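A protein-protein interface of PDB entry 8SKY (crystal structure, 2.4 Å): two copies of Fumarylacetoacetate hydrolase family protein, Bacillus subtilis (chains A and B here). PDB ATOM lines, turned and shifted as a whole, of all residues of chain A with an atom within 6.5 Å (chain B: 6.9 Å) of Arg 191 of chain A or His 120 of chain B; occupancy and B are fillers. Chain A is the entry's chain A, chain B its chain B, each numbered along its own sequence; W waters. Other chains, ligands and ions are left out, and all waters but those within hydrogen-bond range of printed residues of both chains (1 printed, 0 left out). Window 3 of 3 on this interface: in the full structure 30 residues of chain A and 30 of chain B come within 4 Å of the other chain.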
ATOM      1  N   VAL A 144     -13.558 -24.304 -13.578  1.00  0.00           N
ATOM      2  CA  VAL A 144     -14.084 -23.382 -12.599  1.00  0.00           C
ATOM      3  C   VAL A 144     -15.570 -23.240 -12.723  1.00  0.00           C
ATOM      4  O   VAL A 144     -16.214 -22.836 -11.793  1.00  0.00           O
ATOM      5  CB  VAL A 144     -13.399 -22.018 -12.772  1.00  0.00           C
ATOM      6  CG1 VAL A 144     -13.880 -21.273 -13.993  1.00  0.00           C
ATOM      7  CG2 VAL A 144     -13.487 -21.183 -11.513  1.00  0.00           C
ATOM      8  N   ARG A 186     -22.322 -18.431 -15.030  1.00  0.00           N
ATOM      9  CA  ARG A 186     -23.491 -18.135 -14.207  1.00  0.00           C
ATOM     10  C   ARG A 186     -23.290 -18.584 -12.763  1.00  0.00           C
ATOM     11  O   ARG A 186     -23.757 -17.919 -11.831  1.00  0.00           O
ATOM     12  CB  ARG A 186     -24.739 -18.789 -14.808  1.00  0.00           C
ATOM     13  CG  ARG A 186     -25.069 -18.317 -16.220  1.00  0.00           C
ATOM     14  CD  ARG A 186     -25.748 -16.952 -16.219  1.00  0.00           C
ATOM     15  NE  ARG A 186     -26.114 -16.519 -17.566  1.00  0.00           N
ATOM     16  CZ  ARG A 186     -25.979 -15.276 -18.020  1.00  0.00           C
ATOM     17  NH1 ARG A 186     -25.481 -14.329 -17.234  1.00  0.00           N
ATOM     18  NH2 ARG A 186     -26.339 -14.977 -19.261  1.00  0.00           N
ATOM     19  N   ASP A 187     -22.613 -19.713 -12.554  1.00  0.00           N
ATOM     20  CA  ASP A 187     -22.359 -20.168 -11.190  1.00  0.00           C
ATOM     21  C   ASP A 187     -21.419 -19.215 -10.458  1.00  0.00           C
ATOM     22  O   ASP A 187     -21.681 -18.829  -9.314  1.00  0.00           O
ATOM     23  CB  ASP A 187     -21.794 -21.588 -11.198  1.00  0.00           C
ATOM     24  CG  ASP A 187     -20.740 -21.792 -12.264  1.00  0.00           C
ATOM     25  OD1 ASP A 187     -20.399 -20.816 -12.964  1.00  0.00           O
ATOM     26  OD2 ASP A 187     -20.252 -22.933 -12.400  1.00  0.00           O
ATOM     27  N   LEU A 188     -20.318 -18.823 -11.107  1.00  0.00           N
ATOM     28  CA  LEU A 188     -19.380 -17.894 -10.485  1.00  0.00           C
ATOM     29  C   LEU A 188     -20.028 -16.545 -10.217  1.00  0.00           C
ATOM     30  O   LEU A 188     -19.603 -15.818  -9.310  1.00  0.00           O
ATOM     31  CB  LEU A 188     -18.144 -17.712 -11.369  1.00  0.00           C
ATOM     32  CG  LEU A 188     -16.999 -18.723 -11.279  1.00  0.00           C
ATOM     33  CD1 LEU A 188     -17.473 -20.134 -11.582  1.00  0.00           C
ATOM     34  CD2 LEU A 188     -15.885 -18.317 -12.230  1.00  0.00           C
ATOM     35  N   GLN A 189     -21.044 -16.189 -11.004  1.00  0.00           N
ATOM     36  CA  GLN A 189     -21.762 -14.940 -10.782  1.00  0.00           C
ATOM     37  C   GLN A 189     -22.439 -14.934  -9.416  1.00  0.00           C
ATOM     38  O   GLN A 189     -22.387 -13.934  -8.691  1.00  0.00           O
ATOM     39  CB  GLN A 189     -22.784 -14.739 -11.899  1.00  0.00           C
ATOM     40  CG  GLN A 189     -23.230 -13.311 -12.103  1.00  0.00           C
ATOM     41  CD  GLN A 189     -23.877 -13.102 -13.458  1.00  0.00           C
ATOM     42  OE1 GLN A 189     -24.283 -14.059 -14.118  1.00  0.00           O
ATOM     43  NE2 GLN A 189     -23.975 -11.847 -13.880  1.00  0.00           N
ATOM     44  N   LYS A 190     -23.074 -16.049  -9.050  1.00  0.00           N
ATOM     45  CA  LYS A 190     -23.716 -16.144  -7.744  1.00  0.00           C
ATOM     46  C   LYS A 190     -22.694 -16.235  -6.617  1.00  0.00           C
ATOM     47  O   LYS A 190     -22.937 -15.731  -5.514  1.00  0.00           O
ATOM     48  CB  LYS A 190     -24.650 -17.353  -7.704  1.00  0.00           C
ATOM     49  CG  LYS A 190     -26.093 -17.050  -8.055  1.00  0.00           C
ATOM     50  CD  LYS A 190     -26.948 -18.296  -7.908  1.00  0.00           C
ATOM     51  CE  LYS A 190     -28.390 -17.940  -7.600  1.00  0.00           C
ATOM     52  NZ  LYS A 190     -29.143 -17.610  -8.838  1.00  0.00           N
ATOM     53  N   ARG A 191     -21.553 -16.884  -6.868  1.00  0.00           N
ATOM     54  CA  ARG A 191     -20.637 -17.217  -5.780  1.00  0.00           C
ATOM     55  C   ARG A 191     -20.080 -15.970  -5.101  1.00  0.00           C
ATOM     56  O   ARG A 191     -19.991 -15.916  -3.871  1.00  0.00           O
ATOM     57  CB  ARG A 191     -19.498 -18.096  -6.294  1.00  0.00           C
ATOM     58  CG  ARG A 191     -18.905 -18.983  -5.213  1.00  0.00           C
ATOM     59  CD  ARG A 191     -17.588 -19.625  -5.640  1.00  0.00           C
ATOM     60  NE  ARG A 191     -17.723 -20.662  -6.668  1.00  0.00           N
ATOM     61  CZ  ARG A 191     -18.560 -21.700  -6.629  1.00  0.00           C
ATOM     62  NH1 ARG A 191     -19.367 -21.903  -5.594  1.00  0.00           N
ATOM     63  NH2 ARG A 191     -18.575 -22.563  -7.635  1.00  0.00           N
ATOM     64  N   HIS A 192     -19.704 -14.957  -5.877  1.00  0.00           N
ATOM     65  CA  HIS A 192     -19.033 -13.784  -5.339  1.00  0.00           C
ATOM     66  C   HIS A 192     -19.944 -12.567  -5.218  1.00  0.00           C
ATOM     67  O   HIS A 192     -19.486 -11.504  -4.780  1.00  0.00           O
ATOM     68  CB  HIS A 192     -17.795 -13.474  -6.199  1.00  0.00           C
ATOM     69  CG  HIS A 192     -16.890 -14.653  -6.367  1.00  0.00           C
ATOM     70  ND1 HIS A 192     -15.949 -15.005  -5.423  1.00  0.00           N
ATOM     71  CD2 HIS A 192     -16.799 -15.577  -7.350  1.00  0.00           C
ATOM     72  CE1 HIS A 192     -15.310 -16.089  -5.822  1.00  0.00           C
ATOM     73  NE2 HIS A 192     -15.806 -16.457  -6.990  1.00  0.00           N
ATOM     74  N   LYS A 193     -21.196 -12.677  -5.682  1.00  0.00           N
ATOM     75  CA  LYS A 193     -22.321 -11.732  -5.521  1.00  0.00           C
ATOM     76  C   LYS A 193     -22.122 -10.416  -6.263  1.00  0.00           C
ATOM     77  O   LYS A 193     -23.082  -9.709  -6.572  1.00  0.00           O
ATOM     78  CB  LYS A 193     -22.529 -11.371  -4.066  1.00  0.00           C
ATOM     79  CG  LYS A 193     -23.014 -12.457  -3.237  1.00  0.00           C
ATOM     80  CD  LYS A 193     -23.097 -12.009  -1.791  1.00  0.00           C
ATOM     81  CE  LYS A 193     -23.427 -13.204  -0.926  1.00  0.00           C
ATOM     82  NZ  LYS A 193     -24.837 -13.631  -1.227  1.00  0.00           N
ATOM     83  N   GLN A 194     -20.879 -10.103  -6.592  1.00  0.00           N
ATOM     84  CA  GLN A 194     -20.555  -9.021  -7.500  1.00  0.00           C
ATOM     85  C   GLN A 194     -20.143  -9.692  -8.794  1.00  0.00           C
ATOM     86  O   GLN A 194     -19.494 -10.743  -8.778  1.00  0.00           O
ATOM     87  CB  GLN A 194     -19.434  -8.116  -6.964  1.00  0.00           C
ATOM     88  CG  GLN A 194     -19.817  -7.193  -5.798  1.00  0.00           C
ATOM     89  CD  GLN A 194     -20.764  -6.066  -6.195  1.00  0.00           C
ATOM     90  OE1 GLN A 194     -20.487  -5.293  -7.115  1.00  0.00           O
ATOM     91  NE2 GLN A 194     -21.883  -5.965  -5.489  1.00  0.00           N
ATOM     92  N   GLY B 101     -14.330  -7.034  -1.030  1.00  0.00           N
ATOM     93  CA  GLY B 101     -15.380  -6.543  -0.153  1.00  0.00           C
ATOM     94  C   GLY B 101     -15.506  -7.411   1.087  1.00  0.00           C
ATOM     95  O   GLY B 101     -15.391  -8.636   1.015  1.00  0.00           O
ATOM     96  N   ILE B 117     -21.752 -12.375   5.655  1.00  0.00           N
ATOM     97  CA  ILE B 117     -20.286 -12.385   5.462  1.00  0.00           C
ATOM     98  C   ILE B 117     -19.966 -13.425   4.398  1.00  0.00           C
ATOM     99  O   ILE B 117     -20.648 -14.467   4.328  1.00  0.00           O
ATOM    100  CB  ILE B 117     -19.465 -12.669   6.739  1.00  0.00           C
ATOM    101  CG1 ILE B 117     -19.479 -14.151   7.090  1.00  0.00           C
ATOM    102  CG2 ILE B 117     -20.052 -11.919   7.920  1.00  0.00           C
ATOM    103  CD1 ILE B 117     -18.394 -14.514   8.091  1.00  0.00           C
ATOM    104  N   PRO B 118     -19.001 -13.194   3.512  1.00  0.00           N
ATOM    105  CA  PRO B 118     -18.842 -14.105   2.377  1.00  0.00           C
ATOM    106  C   PRO B 118     -17.983 -15.314   2.708  1.00  0.00           C
ATOM    107  O   PRO B 118     -16.951 -15.225   3.375  1.00  0.00           O
ATOM    108  CB  PRO B 118     -18.177 -13.216   1.318  1.00  0.00           C
ATOM    109  CG  PRO B 118     -17.505 -12.108   2.077  1.00  0.00           C
ATOM    110  CD  PRO B 118     -18.005 -12.109   3.499  1.00  0.00           C
ATOM    111  N   GLU B 119     -18.448 -16.470   2.237  1.00  0.00           N
ATOM    112  CA  GLU B 119     -17.685 -17.708   2.284  1.00  0.00           C
ATOM    113  C   GLU B 119     -16.709 -17.825   1.124  1.00  0.00           C
ATOM    114  O   GLU B 119     -15.839 -18.702   1.146  1.00  0.00           O
ATOM    115  CB  GLU B 119     -18.637 -18.907   2.274  1.00  0.00           C
ATOM    116  CG  GLU B 119     -19.845 -18.729   3.175  1.00  0.00           C
ATOM    117  CD  GLU B 119     -20.812 -19.890   3.080  1.00  0.00           C
ATOM    118  OE1 GLU B 119     -20.407 -20.961   2.581  1.00  0.00           O
ATOM    119  OE2 GLU B 119     -21.977 -19.727   3.497  1.00  0.00           O
ATOM    120  N   HIS B 120     -16.852 -16.974   0.116  1.00  0.00           N
ATOM    121  CA  HIS B 120     -15.942 -16.808  -1.000  1.00  0.00           C
ATOM    122  C   HIS B 120     -15.666 -15.323  -1.169  1.00  0.00           C
ATOM    123  O   HIS B 120     -16.526 -14.496  -0.854  1.00  0.00           O
ATOM    124  CB  HIS B 120     -16.537 -17.379  -2.295  1.00  0.00           C
ATOM    125  CG  HIS B 120     -17.172 -18.723  -2.124  1.00  0.00           C
ATOM    126  ND1 HIS B 120     -16.513 -19.899  -2.408  1.00  0.00           N
ATOM    127  CD2 HIS B 120     -18.404 -19.078  -1.687  1.00  0.00           C
ATOM    128  CE1 HIS B 120     -17.312 -20.921  -2.160  1.00  0.00           C
ATOM    129  NE2 HIS B 120     -18.465 -20.450  -1.720  1.00  0.00           N
ATOM    130  N   PRO B 121     -14.480 -14.953  -1.647  1.00  0.00           N
ATOM    131  CA  PRO B 121     -14.161 -13.525  -1.778  1.00  0.00           C
ATOM    132  C   PRO B 121     -15.177 -12.802  -2.650  1.00  0.00           C
ATOM    133  O   PRO B 121     -15.568 -13.282  -3.717  1.00  0.00           O
ATOM    134  CB  PRO B 121     -12.768 -13.532  -2.416  1.00  0.00           C
ATOM    135  CG  PRO B 121     -12.177 -14.827  -1.990  1.00  0.00           C
ATOM    136  CD  PRO B 121     -13.321 -15.805  -1.963  1.00  0.00           C
ATOM    137  N   MET B 122     -15.616 -11.644  -2.168  1.00  0.00           N
ATOM    138  CA  MET B 122     -16.507 -10.759  -2.900  1.00  0.00           C
ATOM    139  C   MET B 122     -15.650  -9.677  -3.543  1.00  0.00           C
ATOM    140  O   MET B 122     -14.981  -8.912  -2.840  1.00  0.00           O
ATOM    141  CB  MET B 122     -17.553 -10.170  -1.956  1.00  0.00           C
ATOM    142  CG  MET B 122     -18.295  -8.955  -2.454  1.00  0.00           C
ATOM    143  SD  MET B 122     -19.622  -8.595  -1.292  1.00  0.00           S
ATOM    144  CE  MET B 122     -19.914  -6.875  -1.641  1.00  0.00           C
ATOM    145  N   VAL B 123     -15.650  -9.632  -4.873  1.00  0.00           N
ATOM    146  CA  VAL B 123     -14.643  -8.893  -5.625  1.00  0.00           C
ATOM    147  C   VAL B 123     -15.321  -7.955  -6.614  1.00  0.00           C
ATOM    148  O   VAL B 123     -16.241  -8.357  -7.335  1.00  0.00           O
ATOM    149  CB  VAL B 123     -13.678  -9.843  -6.359  1.00  0.00           C
ATOM    150  CG1 VAL B 123     -12.623  -9.048  -7.091  1.00  0.00           C
ATOM    151  CG2 VAL B 123     -13.031 -10.805  -5.370  1.00  0.00           C
ATOM    152  N   PHE B 244      -9.601 -14.578   4.253  1.00  0.00           N
ATOM    153  CA  PHE B 244      -8.889 -14.576   2.971  1.00  0.00           C
ATOM    154  C   PHE B 244      -7.556 -13.821   2.956  1.00  0.00           C
ATOM    155  O   PHE B 244      -7.514 -12.656   2.543  1.00  0.00           O
ATOM    156  CB  PHE B 244      -9.760 -14.010   1.847  1.00  0.00           C
ATOM    157  CG  PHE B 244     -11.146 -14.555   1.819  1.00  0.00           C
ATOM    158  CD1 PHE B 244     -11.365 -15.909   1.638  1.00  0.00           C
ATOM    159  CD2 PHE B 244     -12.235 -13.709   1.924  1.00  0.00           C
ATOM    160  CE1 PHE B 244     -12.646 -16.414   1.594  1.00  0.00           C
ATOM    161  CE2 PHE B 244     -13.519 -14.204   1.877  1.00  0.00           C
ATOM    162  CZ  PHE B 244     -13.725 -15.560   1.713  1.00  0.00           C
ATOM    163  N   THR B 252      -7.649 -17.361  -5.494  1.00  0.00           N
ATOM    164  CA  THR B 252      -9.040 -17.254  -5.928  1.00  0.00           C
ATOM    165  C   THR B 252      -9.159 -16.433  -7.208  1.00  0.00           C
ATOM    166  O   THR B 252      -9.801 -16.861  -8.174  1.00  0.00           O
ATOM    167  CB  THR B 252      -9.896 -16.642  -4.815  1.00  0.00           C
ATOM    168  OG1 THR B 252     -10.091 -17.604  -3.771  1.00  0.00           O
ATOM    169  CG2 THR B 252     -11.254 -16.206  -5.354  1.00  0.00           C
HETATM  170  O   HOH W   1     -16.943 -10.587  -8.349  1.00  0.00           O
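A ring nitrogen (ND1) of His 192 of chain A is in hydrogen-bond range of the backbone carbonyl oxygen of Pro 121 of chain B (2.5 Å).
The backbone NH (N) of Gly 101 of chain B sits at hydrogen-bond distance from the backbone carbonyl oxygen (O) of Met 122 of chain B (2.7 Å).
Among the printed residues, merely in contact across the chains: Gln 194 of chain A with Val 123 of chain B (3.2 Å), Arg 191 of chain A with His 120 of chain B (3.4 Å), His 192 of chain A with Met 122 of chain B (3.6 Å) and His 192 of chain A with His 120 of chain B (3.95 Å).
Of chain B, only His 120 comes within 4 Å of Arg 191 of chain A. His 120 of chain B touches two residues of chain A. Of the printed residues of chain B, Gln 194 of chain A touches Val 123 (3.2 Å). Printed residues of chain A within 4 Å of Pro 121 of chain B: His 192. Of the printed residues of chain A, Val 123 of chain B touches Gln 194. Leu 188 of chain A touches none of the printed residues of chain B. Gly 101 of chain B touches none of the printed residues of chain A. The nearest printed residue of chain A that does not touch His 120 of chain B is Lys 190 of chain A (6.8 Å).
Hydrophobic or aromatic side chains of chain A within 4 Å of the printed part of chain B: His 192. Among the printed residues, no Asp or Glu carboxylate lies within 4 Å of a Lys or Arg side-chain nitrogen of the other chain.
No position is printed for both chains.
Water W1 bridges O of Val 123 of chain B and O of Gln 194 of chain A.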
